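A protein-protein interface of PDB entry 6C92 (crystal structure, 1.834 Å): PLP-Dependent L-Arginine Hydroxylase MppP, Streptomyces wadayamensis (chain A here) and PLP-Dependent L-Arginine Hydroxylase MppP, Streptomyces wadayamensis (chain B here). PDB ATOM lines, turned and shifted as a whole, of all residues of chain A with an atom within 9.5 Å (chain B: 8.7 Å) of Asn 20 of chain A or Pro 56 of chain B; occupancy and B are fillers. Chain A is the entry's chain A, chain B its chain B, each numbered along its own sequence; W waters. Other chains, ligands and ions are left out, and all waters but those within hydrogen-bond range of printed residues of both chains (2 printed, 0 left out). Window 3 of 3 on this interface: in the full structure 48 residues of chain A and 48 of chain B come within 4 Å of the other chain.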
ATOM      1  N   TRP A  14       6.178  -6.239  -2.307  1.00  0.00           N
ATOM      2  CA  TRP A  14       7.229  -6.549  -1.334  1.00  0.00           C
ATOM      3  C   TRP A  14       8.316  -5.480  -1.354  1.00  0.00           C
ATOM      4  O   TRP A  14       8.883  -5.139  -0.309  1.00  0.00           O
ATOM      5  CB  TRP A  14       7.869  -7.913  -1.618  1.00  0.00           C
ATOM      6  CG  TRP A  14       7.001  -9.108  -1.409  1.00  0.00           C
ATOM      7  CD1 TRP A  14       6.271  -9.763  -2.357  1.00  0.00           C
ATOM      8  CD2 TRP A  14       6.799  -9.815  -0.181  1.00  0.00           C
ATOM      9  NE1 TRP A  14       5.617 -10.840  -1.790  1.00  0.00           N
ATOM     10  CE2 TRP A  14       5.924 -10.890  -0.455  1.00  0.00           C
ATOM     11  CE3 TRP A  14       7.271  -9.646   1.125  1.00  0.00           C
ATOM     12  CZ2 TRP A  14       5.511 -11.784   0.530  1.00  0.00           C
ATOM     13  CZ3 TRP A  14       6.859 -10.539   2.102  1.00  0.00           C
ATOM     14  CH2 TRP A  14       5.987 -11.593   1.797  1.00  0.00           C
ATOM     15  N   GLU A  15       8.629  -4.949  -2.544  1.00  0.00           N
ATOM     16  CA  GLU A  15       9.711  -3.975  -2.670  1.00  0.00           C
ATOM     17  C   GLU A  15       9.338  -2.632  -2.045  1.00  0.00           C
ATOM     18  O   GLU A  15      10.223  -1.928  -1.540  1.00  0.00           O
ATOM     19  CB  GLU A  15      10.105  -3.813  -4.143  1.00  0.00           C
ATOM     20  CG  GLU A  15      10.822  -5.067  -4.711  1.00  0.00           C
ATOM     21  CD  GLU A  15      11.168  -4.971  -6.196  1.00  0.00           C
ATOM     22  OE1 GLU A  15      10.764  -3.991  -6.856  1.00  0.00           O
ATOM     23  OE2 GLU A  15      11.853  -5.885  -6.708  1.00  0.00           O
ATOM     24  N   TYR A  16       8.047  -2.270  -2.037  1.00  0.00           N
ATOM     25  CA  TYR A  16       7.635  -1.026  -1.374  1.00  0.00           C
ATOM     26  C   TYR A  16       8.001  -1.021   0.102  1.00  0.00           C
ATOM     27  O   TYR A  16       8.277   0.045   0.659  1.00  0.00           O
ATOM     28  CB  TYR A  16       6.129  -0.797  -1.478  1.00  0.00           C
ATOM     29  CG  TYR A  16       5.612  -0.490  -2.858  1.00  0.00           C
ATOM     30  CD1 TYR A  16       6.327   0.326  -3.737  1.00  0.00           C
ATOM     31  CD2 TYR A  16       4.401  -1.009  -3.286  1.00  0.00           C
ATOM     32  CE1 TYR A  16       5.842   0.608  -5.004  1.00  0.00           C
ATOM     33  CE2 TYR A  16       3.906  -0.729  -4.549  1.00  0.00           C
ATOM     34  CZ  TYR A  16       4.644   0.075  -5.404  1.00  0.00           C
ATOM     35  OH  TYR A  16       4.166   0.348  -6.657  1.00  0.00           O
ATOM     36  N   LEU A  17       7.959  -2.181   0.762  1.00  0.00           N
ATOM     37  CA  LEU A  17       8.250  -2.212   2.199  1.00  0.00           C
ATOM     38  C   LEU A  17       9.694  -1.837   2.510  1.00  0.00           C
ATOM     39  O   LEU A  17       9.981  -1.388   3.627  1.00  0.00           O
ATOM     40  CB  LEU A  17       7.955  -3.599   2.775  1.00  0.00           C
ATOM     41  CG  LEU A  17       6.577  -4.193   2.480  1.00  0.00           C
ATOM     42  CD1 LEU A  17       6.531  -5.645   2.948  1.00  0.00           C
ATOM     43  CD2 LEU A  17       5.477  -3.379   3.144  1.00  0.00           C
ATOM     44  N   ALA A  18      10.600  -2.005   1.547  1.00  0.00           N
ATOM     45  CA  ALA A  18      12.024  -1.769   1.747  1.00  0.00           C
ATOM     46  C   ALA A  18      12.469  -0.361   1.369  1.00  0.00           C
ATOM     47  O   ALA A  18      13.594   0.021   1.695  1.00  0.00           O
ATOM     48  CB  ALA A  18      12.829  -2.777   0.917  1.00  0.00           C
ATOM     49  N   LEU A  19      11.608   0.424   0.722  1.00  0.00           N
ATOM     50  CA  LEU A  19      12.071   1.555  -0.081  1.00  0.00           C
ATOM     51  C   LEU A  19      12.681   2.673   0.764  1.00  0.00           C
ATOM     52  O   LEU A  19      13.546   3.409   0.275  1.00  0.00           O
ATOM     53  CB  LEU A  19      10.905   2.090  -0.926  1.00  0.00           C
ATOM     54  CG  LEU A  19      11.148   2.652  -2.330  1.00  0.00           C
ATOM     55  CD1 LEU A  19      12.060   1.762  -3.167  1.00  0.00           C
ATOM     56  CD2 LEU A  19       9.801   2.829  -3.029  1.00  0.00           C
ATOM     57  N   ASN A  20      12.248   2.832   2.015  1.00  0.00           N
ATOM     58  CA  ASN A  20      12.770   3.893   2.867  1.00  0.00           C
ATOM     59  C   ASN A  20      13.685   3.350   3.961  1.00  0.00           C
ATOM     60  O   ASN A  20      13.903   4.030   4.969  1.00  0.00           O
ATOM     61  CB  ASN A  20      11.618   4.708   3.466  1.00  0.00           C
ATOM     62  CG  ASN A  20      10.793   5.437   2.395  1.00  0.00           C
ATOM     63  OD1 ASN A  20      11.249   6.412   1.803  1.00  0.00           O
ATOM     64  ND2 ASN A  20       9.582   4.951   2.137  1.00  0.00           N
ATOM     65  N   SER A  21      14.250   2.155   3.767  1.00  0.00           N
ATOM     66  CA  SER A  21      15.054   1.482   4.778  1.00  0.00           C
ATOM     67  C   SER A  21      16.526   1.431   4.375  1.00  0.00           C
ATOM     68  O   SER A  21      16.867   1.338   3.192  1.00  0.00           O
ATOM     69  CB  SER A  21      14.539   0.059   5.025  1.00  0.00           C
ATOM     70  OG  SER A  21      15.428  -0.659   5.863  1.00  0.00           O
ATOM     71  N   GLU A  22      17.400   1.487   5.387  1.00  0.00           N
ATOM     72  CA  GLU A  22      18.840   1.443   5.145  1.00  0.00           C
ATOM     73  C   GLU A  22      19.273   0.085   4.608  1.00  0.00           C
ATOM     74  O   GLU A  22      20.171   0.004   3.762  1.00  0.00           O
ATOM     75  CB  GLU A  22      19.606   1.762   6.437  1.00  0.00           C
ATOM     76  CG  GLU A  22      21.143   1.662   6.332  1.00  0.00           C
ATOM     77  CD  GLU A  22      21.815   1.293   7.665  1.00  0.00           C
ATOM     78  OE1 GLU A  22      22.995   0.871   7.648  1.00  0.00           O
ATOM     79  OE2 GLU A  22      21.166   1.419   8.726  1.00  0.00           O
ATOM     80  N   LEU A  23      18.682  -0.992   5.112  1.00  0.00           N
ATOM     81  CA  LEU A  23      19.099  -2.339   4.726  1.00  0.00           C
ATOM     82  C   LEU A  23      18.137  -2.943   3.705  1.00  0.00           C
ATOM     83  O   LEU A  23      17.644  -4.059   3.838  1.00  0.00           O
ATOM     84  CB  LEU A  23      19.233  -3.215   5.963  1.00  0.00           C
ATOM     85  CG  LEU A  23      20.340  -2.759   6.928  1.00  0.00           C
ATOM     86  CD1 LEU A  23      20.474  -3.740   8.081  1.00  0.00           C
ATOM     87  CD2 LEU A  23      21.691  -2.595   6.232  1.00  0.00           C
ATOM     88  N   ASN A  24      17.874  -2.154   2.673  1.00  0.00           N
ATOM     89  CA  ASN A  24      17.138  -2.593   1.496  1.00  0.00           C
ATOM     90  C   ASN A  24      18.094  -3.381   0.602  1.00  0.00           C
ATOM     91  O   ASN A  24      19.016  -2.807   0.009  1.00  0.00           O
ATOM     92  CB  ASN A  24      16.556  -1.362   0.792  1.00  0.00           C
ATOM     93  CG  ASN A  24      16.020  -1.669  -0.595  1.00  0.00           C
ATOM     94  OD1 ASN A  24      15.980  -2.823  -0.997  1.00  0.00           O
ATOM     95  ND2 ASN A  24      15.612  -0.628  -1.335  1.00  0.00           N
ATOM     96  N   ALA A  26      16.351  -5.553  -1.504  1.00  0.00           N
ATOM     97  CA  ALA A  26      15.195  -6.115  -2.196  1.00  0.00           C
ATOM     98  C   ALA A  26      15.189  -5.760  -3.683  1.00  0.00           C
ATOM     99  O   ALA A  26      15.554  -6.594  -4.517  1.00  0.00           O
ATOM    100  CB  ALA A  26      13.907  -5.633  -1.524  1.00  0.00           C
ATOM    101  N   ASP A  27      14.779  -4.542  -4.040  1.00  0.00           N
ATOM    102  CA  ASP A  27      14.636  -4.212  -5.451  1.00  0.00           C
ATOM    103  C   ASP A  27      15.994  -4.166  -6.146  1.00  0.00           C
ATOM    104  O   ASP A  27      17.038  -3.912  -5.536  1.00  0.00           O
ATOM    105  CB  ASP A  27      13.892  -2.885  -5.631  1.00  0.00           C
ATOM    106  CG  ASP A  27      14.689  -1.698  -5.147  1.00  0.00           C
ATOM    107  OD1 ASP A  27      15.647  -1.302  -5.848  1.00  0.00           O
ATOM    108  OD2 ASP A  27      14.343  -1.151  -4.075  1.00  0.00           O
ATOM    109  N   ARG A  31      21.682   1.280  -6.499  1.00  0.00           N
ATOM    110  CA  ARG A  31      21.712   2.233  -5.403  1.00  0.00           C
ATOM    111  C   ARG A  31      23.096   2.395  -4.791  1.00  0.00           C
ATOM    112  O   ARG A  31      23.222   3.034  -3.747  1.00  0.00           O
ATOM    113  CB  ARG A  31      20.697   1.818  -4.330  1.00  0.00           C
ATOM    114  CG  ARG A  31      19.267   1.603  -4.941  1.00  0.00           C
ATOM    115  CD  ARG A  31      18.190   1.334  -3.886  1.00  0.00           C
ATOM    116  NE  ARG A  31      16.883   1.044  -4.491  1.00  0.00           N
ATOM    117  CZ  ARG A  31      15.999   1.972  -4.867  1.00  0.00           C
ATOM    118  NH1 ARG A  31      16.259   3.268  -4.713  1.00  0.00           N
ATOM    119  NH2 ARG A  31      14.843   1.609  -5.401  1.00  0.00           N
ATOM    120  N   HIS A 330      15.201  -5.706  10.447  1.00  0.00           N
ATOM    121  CA  HIS A 330      15.170  -4.519   9.597  1.00  0.00           C
ATOM    122  C   HIS A 330      15.913  -4.709   8.282  1.00  0.00           C
ATOM    123  O   HIS A 330      16.325  -3.729   7.660  1.00  0.00           O
ATOM    124  CB  HIS A 330      15.724  -3.299  10.339  1.00  0.00           C
ATOM    125  CG  HIS A 330      15.022  -3.022  11.633  1.00  0.00           C
ATOM    126  ND1 HIS A 330      15.502  -3.463  12.849  1.00  0.00           N
ATOM    127  CD2 HIS A 330      13.864  -2.370  11.898  1.00  0.00           C
ATOM    128  CE1 HIS A 330      14.677  -3.085  13.808  1.00  0.00           C
ATOM    129  NE2 HIS A 330      13.674  -2.423  13.258  1.00  0.00           N
ATOM    130  N   PHE A 332      15.560  -6.171   4.390  1.00  0.00           N
ATOM    131  CA  PHE A 332      14.514  -6.461   3.409  1.00  0.00           C
ATOM    132  C   PHE A 332      15.122  -7.081   2.157  1.00  0.00           C
ATOM    133  O   PHE A 332      15.773  -6.388   1.366  1.00  0.00           O
ATOM    134  CB  PHE A 332      13.733  -5.198   3.065  1.00  0.00           C
ATOM    135  CG  PHE A 332      13.018  -4.614   4.242  1.00  0.00           C
ATOM    136  CD1 PHE A 332      13.670  -3.734   5.092  1.00  0.00           C
ATOM    137  CD2 PHE A 332      11.706  -4.971   4.522  1.00  0.00           C
ATOM    138  CE1 PHE A 332      13.027  -3.214   6.189  1.00  0.00           C
ATOM    139  CE2 PHE A 332      11.058  -4.450   5.622  1.00  0.00           C
ATOM    140  CZ  PHE A 332      11.720  -3.567   6.456  1.00  0.00           C
ATOM    141  N   ALA B  50      22.521  14.961  -4.461  1.00  0.00           N
ATOM    142  CA  ALA B  50      23.021  14.480  -3.181  1.00  0.00           C
ATOM    143  C   ALA B  50      21.901  14.343  -2.155  1.00  0.00           C
ATOM    144  O   ALA B  50      21.844  13.339  -1.429  1.00  0.00           O
ATOM    145  CB  ALA B  50      24.123  15.427  -2.675  1.00  0.00           C
ATOM    146  N   GLU B  51      21.013  15.343  -2.060  1.00  0.00           N
ATOM    147  CA  GLU B  51      19.854  15.224  -1.179  1.00  0.00           C
ATOM    148  C   GLU B  51      19.024  13.986  -1.527  1.00  0.00           C
ATOM    149  O   GLU B  51      18.619  13.220  -0.642  1.00  0.00           O
ATOM    150  CB  GLU B  51      18.980  16.480  -1.268  1.00  0.00           C
ATOM    151  CG  GLU B  51      17.774  16.437  -0.314  1.00  0.00           C
ATOM    152  CD  GLU B  51      16.727  17.533  -0.547  1.00  0.00           C
ATOM    153  OE1 GLU B  51      16.971  18.491  -1.315  1.00  0.00           O
ATOM    154  OE2 GLU B  51      15.642  17.422   0.061  1.00  0.00           O
ATOM    155  N   SER B  52      18.787  13.763  -2.825  1.00  0.00           N
ATOM    156  CA  SER B  52      18.004  12.619  -3.278  1.00  0.00           C
ATOM    157  C   SER B  52      18.686  11.291  -2.970  1.00  0.00           C
ATOM    158  O   SER B  52      17.994  10.292  -2.743  1.00  0.00           O
ATOM    159  CB  SER B  52      17.737  12.744  -4.780  1.00  0.00           C
ATOM    160  OG  SER B  52      16.932  13.867  -5.031  1.00  0.00           O
ATOM    161  N   GLU B  53      20.026  11.258  -2.953  1.00  0.00           N
ATOM    162  CA  GLU B  53      20.750  10.053  -2.542  1.00  0.00           C
ATOM    163  C   GLU B  53      20.640   9.787  -1.043  1.00  0.00           C
ATOM    164  O   GLU B  53      20.749   8.637  -0.615  1.00  0.00           O
ATOM    165  CB  GLU B  53      22.240  10.169  -2.896  1.00  0.00           C
ATOM    166  CG  GLU B  53      22.561  10.048  -4.371  1.00  0.00           C
ATOM    167  CD  GLU B  53      24.039  10.255  -4.668  1.00  0.00           C
ATOM    168  OE1 GLU B  53      24.671  11.120  -4.033  1.00  0.00           O
ATOM    169  OE2 GLU B  53      24.565   9.558  -5.549  1.00  0.00           O
ATOM    170  N   GLN B  54      20.466  10.824  -0.235  1.00  0.00           N
ATOM    171  CA  GLN B  54      20.655  10.706   1.205  1.00  0.00           C
ATOM    172  C   GLN B  54      19.366  10.678   2.018  1.00  0.00           C
ATOM    173  O   GLN B  54      19.385  10.186   3.148  1.00  0.00           O
ATOM    174  CB  GLN B  54      21.536  11.862   1.708  1.00  0.00           C
ATOM    175  CG  GLN B  54      22.974  11.780   1.190  1.00  0.00           C
ATOM    176  CD  GLN B  54      23.743  13.089   1.292  1.00  0.00           C
ATOM    177  OE1 GLN B  54      23.309  14.031   1.951  1.00  0.00           O
ATOM    178  NE2 GLN B  54      24.895  13.149   0.631  1.00  0.00           N
ATOM    179  N   ARG B  55      18.257  11.192   1.490  1.00  0.00           N
ATOM    180  CA  ARG B  55      17.016  11.217   2.250  1.00  0.00           C
ATOM    181  C   ARG B  55      16.076  10.113   1.795  1.00  0.00           C
ATOM    182  O   ARG B  55      16.153   9.659   0.649  1.00  0.00           O
ATOM    183  CB  ARG B  55      16.306  12.565   2.095  1.00  0.00           C
ATOM    184  CG  ARG B  55      17.113  13.737   2.600  1.00  0.00           C
ATOM    185  CD  ARG B  55      16.345  15.050   2.506  1.00  0.00           C
ATOM    186  NE  ARG B  55      15.176  15.022   3.378  1.00  0.00           N
ATOM    187  CZ  ARG B  55      14.093  15.765   3.205  1.00  0.00           C
ATOM    188  NH1 ARG B  55      14.011  16.619   2.198  1.00  0.00           N
ATOM    189  NH2 ARG B  55      13.090  15.656   4.049  1.00  0.00           N
ATOM    190  N   PRO B  56      15.178   9.666   2.674  1.00  0.00           N
ATOM    191  CA  PRO B  56      14.137   8.721   2.249  1.00  0.00           C
ATOM    192  C   PRO B  56      13.221   9.378   1.235  1.00  0.00           C
ATOM    193  O   PRO B  56      12.771  10.511   1.425  1.00  0.00           O
ATOM    194  CB  PRO B  56      13.390   8.388   3.551  1.00  0.00           C
ATOM    195  CG  PRO B  56      14.203   8.997   4.644  1.00  0.00           C
ATOM    196  CD  PRO B  56      14.947  10.136   4.044  1.00  0.00           C
ATOM    197  N   VAL B  57      12.944   8.651   0.153  1.00  0.00           N
ATOM    198  CA  VAL B  57      12.127   9.184  -0.933  1.00  0.00           C
ATOM    199  C   VAL B  57      10.748   9.621  -0.433  1.00  0.00           C
ATOM    200  O   VAL B  57      10.200  10.623  -0.911  1.00  0.00           O
ATOM    201  CB  VAL B  57      12.037   8.137  -2.066  1.00  0.00           C
ATOM    202  CG1 VAL B  57      11.365   6.858  -1.574  1.00  0.00           C
ATOM    203  CG2 VAL B  57      11.334   8.709  -3.282  1.00  0.00           C
ATOM    204  N   GLN B  58      10.184   8.922   0.562  1.00  0.00           N
ATOM    205  CA  GLN B  58       8.848   9.270   1.036  1.00  0.00           C
ATOM    206  C   GLN B  58       8.805  10.704   1.553  1.00  0.00           C
ATOM    207  O   GLN B  58       7.788  11.399   1.416  1.00  0.00           O
ATOM    208  CB  GLN B  58       8.409   8.303   2.138  1.00  0.00           C
ATOM    209  CG  GLN B  58       7.074   8.660   2.775  1.00  0.00           C
ATOM    210  CD  GLN B  58       5.934   8.622   1.762  1.00  0.00           C
ATOM    211  OE1 GLN B  58       5.442   9.660   1.311  1.00  0.00           O
ATOM    212  NE2 GLN B  58       5.521   7.413   1.391  1.00  0.00           N
ATOM    213  N   GLN B  59       9.890  11.154   2.175  1.00  0.00           N
ATOM    214  CA  GLN B  59       9.926  12.513   2.698  1.00  0.00           C
ATOM    215  C   GLN B  59       9.994  13.530   1.570  1.00  0.00           C
ATOM    216  O   GLN B  59       9.298  14.551   1.605  1.00  0.00           O
ATOM    217  CB  GLN B  59      11.124  12.688   3.626  1.00  0.00           C
ATOM    218  CG  GLN B  59      11.042  11.859   4.907  1.00  0.00           C
ATOM    219  CD  GLN B  59      12.215  12.118   5.846  1.00  0.00           C
ATOM    220  OE1 GLN B  59      12.988  13.066   5.654  1.00  0.00           O
ATOM    221  NE2 GLN B  59      12.358  11.271   6.861  1.00  0.00           N
ATOM    222  N   ILE B  60      10.837  13.275   0.568  1.00  0.00           N
ATOM    223  CA  ILE B  60      10.918  14.174  -0.576  1.00  0.00           C
ATOM    224  C   ILE B  60       9.584  14.196  -1.306  1.00  0.00           C
ATOM    225  O   ILE B  60       9.069  15.272  -1.652  1.00  0.00           O
ATOM    226  CB  ILE B  60      12.080  13.765  -1.498  1.00  0.00           C
ATOM    227  CG1 ILE B  60      13.404  13.849  -0.719  1.00  0.00           C
ATOM    228  CG2 ILE B  60      12.135  14.682  -2.722  1.00  0.00           C
ATOM    229  CD1 ILE B  60      14.590  13.282  -1.489  1.00  0.00           C
ATOM    230  N   GLU B  61       8.979  13.012  -1.503  1.00  0.00           N
ATOM    231  CA  GLU B  61       7.680  12.934  -2.165  1.00  0.00           C
ATOM    232  C   GLU B  61       6.619  13.714  -1.400  1.00  0.00           C
ATOM    233  O   GLU B  61       5.843  14.476  -1.988  1.00  0.00           O
ATOM    234  CB  GLU B  61       7.246  11.479  -2.315  1.00  0.00           C
ATOM    235  CG  GLU B  61       5.952  11.341  -3.118  1.00  0.00           C
ATOM    236  CD  GLU B  61       5.474   9.911  -3.296  1.00  0.00           C
ATOM    237  OE1 GLU B  61       4.799   9.621  -4.320  1.00  0.00           O
ATOM    238  OE2 GLU B  61       5.739   9.083  -2.403  1.00  0.00           O
ATOM    239  N   SER B  62       6.575  13.539  -0.076  1.00  0.00           N
ATOM    240  CA  SER B  62       5.592  14.255   0.730  1.00  0.00           C
ATOM    241  C   SER B  62       5.758  15.758   0.593  1.00  0.00           C
ATOM    242  O   SER B  62       4.765  16.495   0.506  1.00  0.00           O
ATOM    243  CB  SER B  62       5.713  13.843   2.197  1.00  0.00           C
ATOM    244  OG  SER B  62       5.054  12.611   2.425  1.00  0.00           O
ATOM    245  N   GLU B  63       7.005  16.232   0.563  1.00  0.00           N
ATOM    246  CA  GLU B  63       7.255  17.671   0.426  1.00  0.00           C
ATOM    247  C   GLU B  63       6.872  18.184  -0.955  1.00  0.00           C
ATOM    248  O   GLU B  63       6.343  19.297  -1.093  1.00  0.00           O
ATOM    249  CB  GLU B  63       8.727  17.974   0.701  1.00  0.00           C
ATOM    250  CG  GLU B  63       9.125  17.683   2.133  1.00  0.00           C
ATOM    251  CD  GLU B  63      10.631  17.596   2.359  1.00  0.00           C
ATOM    252  OE1 GLU B  63      11.022  17.345   3.509  1.00  0.00           O
ATOM    253  OE2 GLU B  63      11.422  17.766   1.406  1.00  0.00           O
ATOM    254  N   PRO B  81       0.391   8.865   3.187  1.00  0.00           N
ATOM    255  CA  PRO B  81       1.180   8.135   2.182  1.00  0.00           C
ATOM    256  C   PRO B  81       0.359   7.064   1.467  1.00  0.00           C
ATOM    257  O   PRO B  81      -0.420   6.333   2.081  1.00  0.00           O
ATOM    258  CB  PRO B  81       2.316   7.520   3.006  1.00  0.00           C
ATOM    259  CG  PRO B  81       2.456   8.437   4.185  1.00  0.00           C
ATOM    260  CD  PRO B  81       1.065   8.903   4.498  1.00  0.00           C
ATOM    261  N   PRO B 256      13.489  10.323  -7.064  1.00  0.00           N
ATOM    262  CA  PRO B 256      13.517  11.368  -6.029  1.00  0.00           C
ATOM    263  C   PRO B 256      14.008  12.711  -6.542  1.00  0.00           C
ATOM    264  O   PRO B 256      13.607  13.755  -5.999  1.00  0.00           O
ATOM    265  CB  PRO B 256      14.449  10.785  -4.957  1.00  0.00           C
ATOM    266  CG  PRO B 256      15.267   9.789  -5.655  1.00  0.00           C
ATOM    267  CD  PRO B 256      14.330   9.176  -6.694  1.00  0.00           C
ATOM    268  N   LEU B 259      11.060  14.552  -7.993  1.00  0.00           N
ATOM    269  CA  LEU B 259      10.202  15.026  -6.905  1.00  0.00           C
ATOM    270  C   LEU B 259      10.815  16.243  -6.220  1.00  0.00           C
ATOM    271  O   LEU B 259      10.113  17.206  -5.882  1.00  0.00           O
ATOM    272  CB  LEU B 259       9.973  13.892  -5.911  1.00  0.00           C
ATOM    273  CG  LEU B 259       9.096  12.734  -6.425  1.00  0.00           C
ATOM    274  CD1 LEU B 259       9.297  11.522  -5.532  1.00  0.00           C
ATOM    275  CD2 LEU B 259       7.634  13.171  -6.505  1.00  0.00           C
ATOM    276  N   ARG B 263       9.265  19.981  -6.004  1.00  0.00           N
ATOM    277  CA  ARG B 263       9.223  20.752  -4.761  1.00  0.00           C
ATOM    278  C   ARG B 263       9.831  22.142  -4.951  1.00  0.00           C
ATOM    279  O   ARG B 263       9.254  23.155  -4.530  1.00  0.00           O
ATOM    280  CB  ARG B 263       9.955  19.982  -3.667  1.00  0.00           C
ATOM    281  CG  ARG B 263       9.966  20.679  -2.291  1.00  0.00           C
ATOM    282  CD  ARG B 263      10.968  20.039  -1.384  1.00  0.00           C
ATOM    283  NE  ARG B 263      12.333  20.270  -1.853  1.00  0.00           N
ATOM    284  CZ  ARG B 263      13.375  19.509  -1.552  1.00  0.00           C
ATOM    285  NH1 ARG B 263      13.246  18.438  -0.785  1.00  0.00           N
ATOM    286  NH2 ARG B 263      14.559  19.815  -2.049  1.00  0.00           N
HETATM  287  O   HOH W   1      14.386   6.067  -0.021  1.00  0.00           O
HETATM  288  O   HOH W   2       7.558   5.488  -0.030  1.00  0.00           O
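The backbone NH of Gln 58 of chain B lies within hydrogen-bond range of the side-chain amide oxygen of Asn 20 of chain A, at 3.0 Å. The side-chain amide oxygen of Asn 20 of chain A lies within hydrogen-bond range of the backbone NH of Val 57 of chain B (3.3 Å).
OG of Ser 62 of chain B is in hydrogen-bond range of O of Gln 58 of chain B (3.2 Å).
Among the printed residues, pairs that only touch across the chains: Asn 20 of chain A with Pro 56 of chain B (3.4 Å).
Of chain A, only Asn 20 comes within 4 Å of Pro 56 of chain B. Of chain A, only Asn 20 (3.3 Å) comes within 4 Å of Val 57 of chain B. Printed residues of chain A within 4 Å of Gln 58 of chain B: Asn 20 (3.0 Å). Ile 60 of chain B touches none of the printed residues of chain A. Pro 256 of chain B touches none of the printed residues of chain A. The nearest residue of chain B that does not touch Asn 20 of chain A is Gln 59 of chain B (4.9 Å). The nearest printed residue of chain A that does not touch Gln 58 of chain B is Leu 19 of chain A (6.5 Å).
Among the printed residues, 3 pairs touch across the chains.
Water W1 lies within hydrogen-bond range of the backbone carbonyl oxygen of Leu 19 of chain A and the backbone NH of Val 57 of chain B. Water W2 bridges the side-chain amide nitrogen of Asn 20 of chain A (3.0 Å) and the side-chain amide nitrogen of Gln 58 of chain B (3.1 Å).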
